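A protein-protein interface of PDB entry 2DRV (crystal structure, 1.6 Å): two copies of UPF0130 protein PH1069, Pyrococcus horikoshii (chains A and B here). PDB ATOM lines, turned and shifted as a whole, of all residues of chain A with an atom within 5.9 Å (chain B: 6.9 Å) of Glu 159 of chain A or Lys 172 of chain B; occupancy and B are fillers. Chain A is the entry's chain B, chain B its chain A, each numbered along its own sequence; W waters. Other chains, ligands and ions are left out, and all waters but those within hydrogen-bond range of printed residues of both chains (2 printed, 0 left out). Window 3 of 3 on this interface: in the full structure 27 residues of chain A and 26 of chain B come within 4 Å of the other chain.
O of Leu 156 of chain A lies within hydrogen-bond range of OH of Tyr 169 of chain B (2.7 Å).
N of Phe 164 of chain A lies within hydrogen-bond range of O of Leu 157 of chain A (2.7 Å).
Among the printed residues, merely in contact across the chains: Gln 98 of chain A with Ile 176 of chain B, Leu 156 of chain A with Ile 173 of chain B, Glu 159 of chain A with Lys 172 of chain B and Phe 164 of chain A with Tyr 169 of chain B.
Of the printed residues of chain B, Gln 98 of chain A touches Ile 176 (3.5 Å). Glu 159 of chain A touches just one residue of chain B: Lys 172 (3.7 Å). Of the printed residues of chain A, Tyr 169 of chain B touches Leu 156 (2.7 Å) and Phe 164 (3.9 Å). Of chain A, only Glu 159 (3.7 Å) comes within 4 Å of Lys 172 of chain B. Printed residues of chain A within 4 Å of Ile 176 of chain B: Gln 98 (3.5 Å). The nearest residue of chain B that does not touch Glu 159 of chain A is Ile 176 of chain B (4.2 Å).
Hydrophobic or aromatic side chains of chain A within 4 Å of the printed part of chain B: Leu 156 and Phe 164. Printed residues of chain B that touch a printed residue of chain A: Tyr 169, Lys 172, Ile 173 and Ile 176. Hydrophobic or aromatic side chains of chain B that line the printed part of chain A: Tyr 169, Ile 173 and Ile 176. Among the printed residues, 5 pairs touch across the chains. Among the printed residues, no Asp or Glu carboxylate lies within 4 Å of a Lys or Arg side-chain nitrogen of the other chain.
No position is printed for both chains.
Water W1 bridges the side-chain amino group of Lys 172 of chain B (2.5 Å) and the side-chain carboxylate of Glu 159 of chain A (3.5 Å). Water W2 bridges the backbone carbonyl oxygen (O) of Lys 172 of chain B and the side-chain carboxylate (OE2) of Glu 159 of chain A.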
ATOM      1  N   HIS A  94     -21.688   8.643  27.918  1.00  0.00           N
ATOM      2  CA  HIS A  94     -21.948   9.085  26.551  1.00  0.00           C
ATOM      3  C   HIS A  94     -20.698   9.563  25.826  1.00  0.00           C
ATOM      4  O   HIS A  94     -19.917  10.346  26.370  1.00  0.00           O
ATOM      5  CB  HIS A  94     -22.979  10.213  26.541  1.00  0.00           C
ATOM      6  CG  HIS A  94     -23.196  10.805  25.184  1.00  0.00           C
ATOM      7  ND1 HIS A  94     -23.431  10.040  24.063  1.00  0.00           N
ATOM      8  CD2 HIS A  94     -23.231  12.095  24.774  1.00  0.00           C
ATOM      9  CE1 HIS A  94     -23.599  10.835  23.019  1.00  0.00           C
ATOM     10  NE2 HIS A  94     -23.484  12.086  23.426  1.00  0.00           N
ATOM     11  N   SER A  96     -20.633   9.044  21.747  1.00  0.00           N
ATOM     12  CA  SER A  96     -20.918   9.209  20.322  1.00  0.00           C
ATOM     13  C   SER A  96     -22.388   9.198  19.928  1.00  0.00           C
ATOM     14  O   SER A  96     -23.217   8.577  20.592  1.00  0.00           O
ATOM     15  CB  SER A  96     -20.182   8.121  19.531  1.00  0.00           C
ATOM     16  OG  SER A  96     -20.513   8.163  18.150  1.00  0.00           O
ATOM     17  N   GLY A  97     -22.689   9.889  18.830  1.00  0.00           N
ATOM     18  CA  GLY A  97     -24.046   9.953  18.316  1.00  0.00           C
ATOM     19  C   GLY A  97     -24.989  10.790  19.153  1.00  0.00           C
ATOM     20  O   GLY A  97     -24.559  11.577  19.996  1.00  0.00           O
ATOM     21  N   GLN A  98     -26.285  10.635  18.909  1.00  0.00           N
ATOM     22  CA  GLN A  98     -27.276  11.375  19.680  1.00  0.00           C
ATOM     23  C   GLN A  98     -27.539  10.590  20.957  1.00  0.00           C
ATOM     24  O   GLN A  98     -27.701   9.368  20.914  1.00  0.00           O
ATOM     25  CB  GLN A  98     -28.588  11.518  18.899  1.00  0.00           C
ATOM     26  CG  GLN A  98     -28.443  12.142  17.517  1.00  0.00           C
ATOM     27  CD  GLN A  98     -29.748  12.168  16.745  1.00  0.00           C
ATOM     28  OE1 GLN A  98     -30.662  11.390  17.019  1.00  0.00           O
ATOM     29  NE2 GLN A  98     -29.834  13.051  15.755  1.00  0.00           N
ATOM     30  N   LEU A  99     -27.568  11.287  22.089  1.00  0.00           N
ATOM     31  CA  LEU A  99     -27.847  10.652  23.374  1.00  0.00           C
ATOM     32  C   LEU A  99     -29.323  10.892  23.650  1.00  0.00           C
ATOM     33  O   LEU A  99     -29.784  12.026  23.631  1.00  0.00           O
ATOM     34  CB  LEU A  99     -27.004  11.283  24.488  1.00  0.00           C
ATOM     35  CG  LEU A  99     -27.174  10.670  25.885  1.00  0.00           C
ATOM     36  CD1 LEU A  99     -26.713   9.211  25.885  1.00  0.00           C
ATOM     37  CD2 LEU A  99     -26.372  11.487  26.893  1.00  0.00           C
ATOM     38  N   LEU A 156     -33.898  14.351  23.854  1.00  0.00           N
ATOM     39  CA  LEU A 156     -32.510  14.447  23.434  1.00  0.00           C
ATOM     40  C   LEU A 156     -31.717  14.977  24.620  1.00  0.00           C
ATOM     41  O   LEU A 156     -32.065  16.007  25.186  1.00  0.00           O
ATOM     42  CB  LEU A 156     -32.391  15.411  22.253  1.00  0.00           C
ATOM     43  CG  LEU A 156     -30.998  15.626  21.652  1.00  0.00           C
ATOM     44  CD1 LEU A 156     -30.472  14.311  21.095  1.00  0.00           C
ATOM     45  CD2 LEU A 156     -31.076  16.676  20.537  1.00  0.00           C
ATOM     46  N   LEU A 157     -30.664  14.264  25.005  1.00  0.00           N
ATOM     47  CA  LEU A 157     -29.857  14.686  26.143  1.00  0.00           C
ATOM     48  C   LEU A 157     -28.534  15.307  25.728  1.00  0.00           C
ATOM     49  O   LEU A 157     -27.949  16.085  26.478  1.00  0.00           O
ATOM     50  CB  LEU A 157     -29.578  13.501  27.067  1.00  0.00           C
ATOM     51  CG  LEU A 157     -30.797  12.853  27.722  1.00  0.00           C
ATOM     52  CD1 LEU A 157     -30.348  11.695  28.596  1.00  0.00           C
ATOM     53  CD2 LEU A 157     -31.551  13.895  28.541  1.00  0.00           C
ATOM     54  N   GLY A 158     -28.067  14.966  24.532  1.00  0.00           N
ATOM     55  CA  GLY A 158     -26.800  15.496  24.061  1.00  0.00           C
ATOM     56  C   GLY A 158     -26.416  14.875  22.737  1.00  0.00           C
ATOM     57  O   GLY A 158     -27.170  14.075  22.185  1.00  0.00           O
ATOM     58  N   GLU A 159     -25.250  15.247  22.218  1.00  0.00           N
ATOM     59  CA  GLU A 159     -24.778  14.706  20.944  1.00  0.00           C
ATOM     60  C   GLU A 159     -23.259  14.707  20.840  1.00  0.00           C
ATOM     61  O   GLU A 159     -22.607  15.681  21.213  1.00  0.00           O
ATOM     62  CB  GLU A 159     -25.333  15.515  19.768  1.00  0.00           C
ATOM     63  CG  GLU A 159     -26.845  15.580  19.681  1.00  0.00           C
ATOM     64  CD  GLU A 159     -27.327  16.245  18.410  1.00  0.00           C
ATOM     65  OE1 GLU A 159     -26.703  17.241  17.981  1.00  0.00           O
ATOM     66  OE2 GLU A 159     -28.340  15.780  17.845  1.00  0.00           O
ATOM     67  N   ASN A 160     -22.707  13.611  20.325  1.00  0.00           N
ATOM     68  CA  ASN A 160     -21.265  13.468  20.127  1.00  0.00           C
ATOM     69  C   ASN A 160     -20.430  13.760  21.371  1.00  0.00           C
ATOM     70  O   ASN A 160     -19.324  14.302  21.277  1.00  0.00           O
ATOM     71  CB  ASN A 160     -20.821  14.372  18.973  1.00  0.00           C
ATOM     72  CG  ASN A 160     -19.395  14.097  18.523  1.00  0.00           C
ATOM     73  OD1 ASN A 160     -18.983  12.941  18.389  1.00  0.00           O
ATOM     74  ND2 ASN A 160     -18.640  15.161  18.272  1.00  0.00           N
ATOM     75  N   GLY A 161     -20.956  13.393  22.533  1.00  0.00           N
ATOM     76  CA  GLY A 161     -20.233  13.613  23.771  1.00  0.00           C
ATOM     77  C   GLY A 161     -20.668  14.847  24.536  1.00  0.00           C
ATOM     78  O   GLY A 161     -20.444  14.933  25.737  1.00  0.00           O
ATOM     79  N   GLU A 162     -21.285  15.802  23.846  1.00  0.00           N
ATOM     80  CA  GLU A 162     -21.747  17.029  24.487  1.00  0.00           C
ATOM     81  C   GLU A 162     -23.120  16.818  25.104  1.00  0.00           C
ATOM     82  O   GLU A 162     -23.999  16.237  24.475  1.00  0.00           O
ATOM     83  CB  GLU A 162     -21.835  18.163  23.468  1.00  0.00           C
ATOM     84  CG  GLU A 162     -22.154  19.515  24.086  1.00  0.00           C
ATOM     85  CD  GLU A 162     -22.379  20.593  23.046  1.00  0.00           C
ATOM     86  OE1 GLU A 162     -21.644  20.609  22.036  1.00  0.00           O
ATOM     87  OE2 GLU A 162     -23.284  21.432  23.245  1.00  0.00           O
ATOM     88  N   ILE A 163     -23.303  17.299  26.330  1.00  0.00           N
ATOM     89  CA  ILE A 163     -24.579  17.168  27.028  1.00  0.00           C
ATOM     90  C   ILE A 163     -25.333  18.497  26.903  1.00  0.00           C
ATOM     91  O   ILE A 163     -24.752  19.566  27.076  1.00  0.00           O
ATOM     92  CB  ILE A 163     -24.342  16.814  28.518  1.00  0.00           C
ATOM     93  CG1 ILE A 163     -23.510  15.528  28.607  1.00  0.00           C
ATOM     94  CG2 ILE A 163     -25.667  16.670  29.263  1.00  0.00           C
ATOM     95  CD1 ILE A 163     -24.070  14.360  27.812  1.00  0.00           C
ATOM     96  N   PHE A 164     -26.624  18.424  26.602  1.00  0.00           N
ATOM     97  CA  PHE A 164     -27.429  19.628  26.416  1.00  0.00           C
ATOM     98  C   PHE A 164     -28.270  20.036  27.618  1.00  0.00           C
ATOM     99  O   PHE A 164     -28.710  21.184  27.707  1.00  0.00           O
ATOM    100  CB  PHE A 164     -28.380  19.460  25.224  1.00  0.00           C
ATOM    101  CG  PHE A 164     -27.702  19.104  23.926  1.00  0.00           C
ATOM    102  CD1 PHE A 164     -26.452  19.619  23.602  1.00  0.00           C
ATOM    103  CD2 PHE A 164     -28.342  18.279  23.007  1.00  0.00           C
ATOM    104  CE1 PHE A 164     -25.849  19.320  22.382  1.00  0.00           C
ATOM    105  CE2 PHE A 164     -27.751  17.973  21.785  1.00  0.00           C
ATOM    106  CZ  PHE A 164     -26.500  18.495  21.469  1.00  0.00           C
ATOM    107  N   LEU B  84     -38.133  26.696  12.747  1.00  0.00           N
ATOM    108  CA  LEU B  84     -37.872  26.967  14.154  1.00  0.00           C
ATOM    109  C   LEU B  84     -38.789  28.011  14.775  1.00  0.00           C
ATOM    110  O   LEU B  84     -39.325  27.811  15.859  1.00  0.00           O
ATOM    111  CB  LEU B  84     -36.419  27.420  14.340  1.00  0.00           C
ATOM    112  CG  LEU B  84     -36.010  27.770  15.773  1.00  0.00           C
ATOM    113  CD1 LEU B  84     -36.053  26.516  16.637  1.00  0.00           C
ATOM    114  CD2 LEU B  84     -34.613  28.370  15.780  1.00  0.00           C
ATOM    115  N   GLU B 167     -33.390  27.866  22.656  1.00  0.00           N
ATOM    116  CA  GLU B 167     -33.561  27.931  21.210  1.00  0.00           C
ATOM    117  C   GLU B 167     -32.665  26.982  20.421  1.00  0.00           C
ATOM    118  O   GLU B 167     -33.109  26.363  19.460  1.00  0.00           O
ATOM    119  CB  GLU B 167     -33.341  29.366  20.709  1.00  0.00           C
ATOM    120  CG  GLU B 167     -33.831  29.587  19.282  1.00  0.00           C
ATOM    121  CD  GLU B 167     -33.703  31.030  18.818  1.00  0.00           C
ATOM    122  OE1 GLU B 167     -34.212  31.932  19.517  1.00  0.00           O
ATOM    123  OE2 GLU B 167     -33.101  31.260  17.748  1.00  0.00           O
ATOM    124  N   GLU B 168     -31.400  26.876  20.811  1.00  0.00           N
ATOM    125  CA  GLU B 168     -30.489  25.984  20.106  1.00  0.00           C
ATOM    126  C   GLU B 168     -30.982  24.547  20.224  1.00  0.00           C
ATOM    127  O   GLU B 168     -30.945  23.789  19.257  1.00  0.00           O
ATOM    128  CB  GLU B 168     -29.076  26.097  20.680  1.00  0.00           C
ATOM    129  CG  GLU B 168     -28.095  25.101  20.084  1.00  0.00           C
ATOM    130  CD  GLU B 168     -26.667  25.366  20.510  1.00  0.00           C
ATOM    131  OE1 GLU B 168     -26.106  26.402  20.096  1.00  0.00           O
ATOM    132  OE2 GLU B 168     -26.106  24.542  21.262  1.00  0.00           O
ATOM    133  N   TYR B 169     -31.452  24.185  21.412  1.00  0.00           N
ATOM    134  CA  TYR B 169     -31.962  22.837  21.642  1.00  0.00           C
ATOM    135  C   TYR B 169     -33.166  22.583  20.743  1.00  0.00           C
ATOM    136  O   TYR B 169     -33.247  21.551  20.079  1.00  0.00           O
ATOM    137  CB  TYR B 169     -32.380  22.664  23.097  1.00  0.00           C
ATOM    138  CG  TYR B 169     -32.864  21.270  23.437  1.00  0.00           C
ATOM    139  CD1 TYR B 169     -31.967  20.275  23.824  1.00  0.00           C
ATOM    140  CD2 TYR B 169     -34.220  20.951  23.385  1.00  0.00           C
ATOM    141  CE1 TYR B 169     -32.409  18.996  24.161  1.00  0.00           C
ATOM    142  CE2 TYR B 169     -34.674  19.672  23.716  1.00  0.00           C
ATOM    143  CZ  TYR B 169     -33.763  18.704  24.105  1.00  0.00           C
ATOM    144  OH  TYR B 169     -34.211  17.456  24.468  1.00  0.00           O
ATOM    145  N   LEU B 170     -34.104  23.524  20.730  1.00  0.00           N
ATOM    146  CA  LEU B 170     -35.299  23.376  19.903  1.00  0.00           C
ATOM    147  C   LEU B 170     -34.928  23.267  18.432  1.00  0.00           C
ATOM    148  O   LEU B 170     -35.563  22.536  17.678  1.00  0.00           O
ATOM    149  CB  LEU B 170     -36.253  24.553  20.137  1.00  0.00           C
ATOM    150  CG  LEU B 170     -36.914  24.538  21.519  1.00  0.00           C
ATOM    151  CD1 LEU B 170     -37.608  25.860  21.790  1.00  0.00           C
ATOM    152  CD2 LEU B 170     -37.903  23.385  21.590  1.00  0.00           C
ATOM    153  N   ASN B 171     -33.887  23.982  18.017  1.00  0.00           N
ATOM    154  CA  ASN B 171     -33.465  23.920  16.627  1.00  0.00           C
ATOM    155  C   ASN B 171     -33.027  22.495  16.305  1.00  0.00           C
ATOM    156  O   ASN B 171     -33.278  21.987  15.213  1.00  0.00           O
ATOM    157  CB  ASN B 171     -32.314  24.891  16.369  1.00  0.00           C
ATOM    158  CG  ASN B 171     -31.919  24.941  14.910  1.00  0.00           C
ATOM    159  OD1 ASN B 171     -30.767  24.679  14.560  1.00  0.00           O
ATOM    160  ND2 ASN B 171     -32.868  25.281  14.050  1.00  0.00           N
ATOM    161  N   LYS B 172     -32.367  21.851  17.261  1.00  0.00           N
ATOM    162  CA  LYS B 172     -31.913  20.483  17.064  1.00  0.00           C
ATOM    163  C   LYS B 172     -33.110  19.541  16.979  1.00  0.00           C
ATOM    164  O   LYS B 172     -33.143  18.649  16.136  1.00  0.00           O
ATOM    165  CB  LYS B 172     -30.991  20.058  18.208  1.00  0.00           C
ATOM    166  CG  LYS B 172     -29.623  20.727  18.181  1.00  0.00           C
ATOM    167  CD  LYS B 172     -28.767  20.182  17.045  1.00  0.00           C
ATOM    168  CE  LYS B 172     -27.487  20.983  16.869  1.00  0.00           C
ATOM    169  NZ  LYS B 172     -27.279  21.420  15.458  1.00  0.00           N
ATOM    170  N   ILE B 173     -34.091  19.744  17.853  1.00  0.00           N
ATOM    171  CA  ILE B 173     -35.286  18.904  17.853  1.00  0.00           C
ATOM    172  C   ILE B 173     -36.035  19.064  16.532  1.00  0.00           C
ATOM    173  O   ILE B 173     -36.552  18.093  15.977  1.00  0.00           O
ATOM    174  CB  ILE B 173     -36.235  19.273  19.025  1.00  0.00           C
ATOM    175  CG1 ILE B 173     -35.569  18.935  20.363  1.00  0.00           C
ATOM    176  CG2 ILE B 173     -37.574  18.549  18.876  1.00  0.00           C
ATOM    177  CD1 ILE B 173     -35.277  17.463  20.549  1.00  0.00           C
ATOM    178  N   VAL B 174     -36.093  20.294  16.030  1.00  0.00           N
ATOM    179  CA  VAL B 174     -36.780  20.560  14.773  1.00  0.00           C
ATOM    180  C   VAL B 174     -36.065  19.874  13.614  1.00  0.00           C
ATOM    181  O   VAL B 174     -36.711  19.302  12.740  1.00  0.00           O
ATOM    182  CB  VAL B 174     -36.890  22.085  14.501  1.00  0.00           C
ATOM    183  CG1 VAL B 174     -37.296  22.337  13.053  1.00  0.00           C
ATOM    184  CG2 VAL B 174     -37.914  22.697  15.433  1.00  0.00           C
ATOM    185  N   GLU B 175     -34.735  19.920  13.606  1.00  0.00           N
ATOM    186  CA  GLU B 175     -33.981  19.278  12.540  1.00  0.00           C
ATOM    187  C   GLU B 175     -34.290  17.783  12.524  1.00  0.00           C
ATOM    188  O   GLU B 175     -34.549  17.202  11.470  1.00  0.00           O
ATOM    189  CB  GLU B 175     -32.477  19.497  12.735  1.00  0.00           C
ATOM    190  CG  GLU B 175     -31.617  18.780  11.703  1.00  0.00           C
ATOM    191  CD  GLU B 175     -30.169  19.228  11.728  1.00  0.00           C
ATOM    192  OE1 GLU B 175     -29.911  20.422  11.461  1.00  0.00           O
ATOM    193  OE2 GLU B 175     -29.288  18.389  12.012  1.00  0.00           O
ATOM    194  N   ILE B 176     -34.272  17.168  13.705  1.00  0.00           N
ATOM    195  CA  ILE B 176     -34.547  15.744  13.824  1.00  0.00           C
ATOM    196  C   ILE B 176     -35.989  15.411  13.437  1.00  0.00           C
ATOM    197  O   ILE B 176     -36.233  14.411  12.764  1.00  0.00           O
ATOM    198  CB  ILE B 176     -34.247  15.252  15.258  1.00  0.00           C
ATOM    199  CG1 ILE B 176     -32.745  15.400  15.534  1.00  0.00           C
ATOM    200  CG2 ILE B 176     -34.680  13.801  15.424  1.00  0.00           C
ATOM    201  CD1 ILE B 176     -32.347  15.131  16.966  1.00  0.00           C
ATOM    202  N   ALA B 177     -36.936  16.247  13.849  1.00  0.00           N
ATOM    203  CA  ALA B 177     -38.342  16.024  13.512  1.00  0.00           C
ATOM    204  C   ALA B 177     -38.536  16.039  11.997  1.00  0.00           C
ATOM    205  O   ALA B 177     -39.212  15.174  11.439  1.00  0.00           O
ATOM    206  CB  ALA B 177     -39.216  17.091  14.157  1.00  0.00           C
ATOM    207  N   ASP B 179     -36.359  15.372   9.792  1.00  0.00           N
ATOM    208  CA  ASP B 179     -35.732  14.210   9.181  1.00  0.00           C
ATOM    209  C   ASP B 179     -36.702  13.046   9.222  1.00  0.00           C
ATOM    210  O   ASP B 179     -36.741  12.238   8.305  1.00  0.00           O
ATOM    211  CB  ASP B 179     -34.531  13.776  10.010  1.00  0.00           C
ATOM    212  CG  ASP B 179     -33.265  14.617   9.765  1.00  0.00           C
ATOM    213  OD1 ASP B 179     -33.081  15.098   8.652  1.00  0.00           O
ATOM    214  OD2 ASP B 179     -32.484  14.744  10.705  1.00  0.00           O
HETATM  215  O   HOH W   1     -26.891  19.040  14.993  1.00  0.00           O
HETATM  216  O   HOH W   2     -30.112  17.703  15.799  1.00  0.00           O
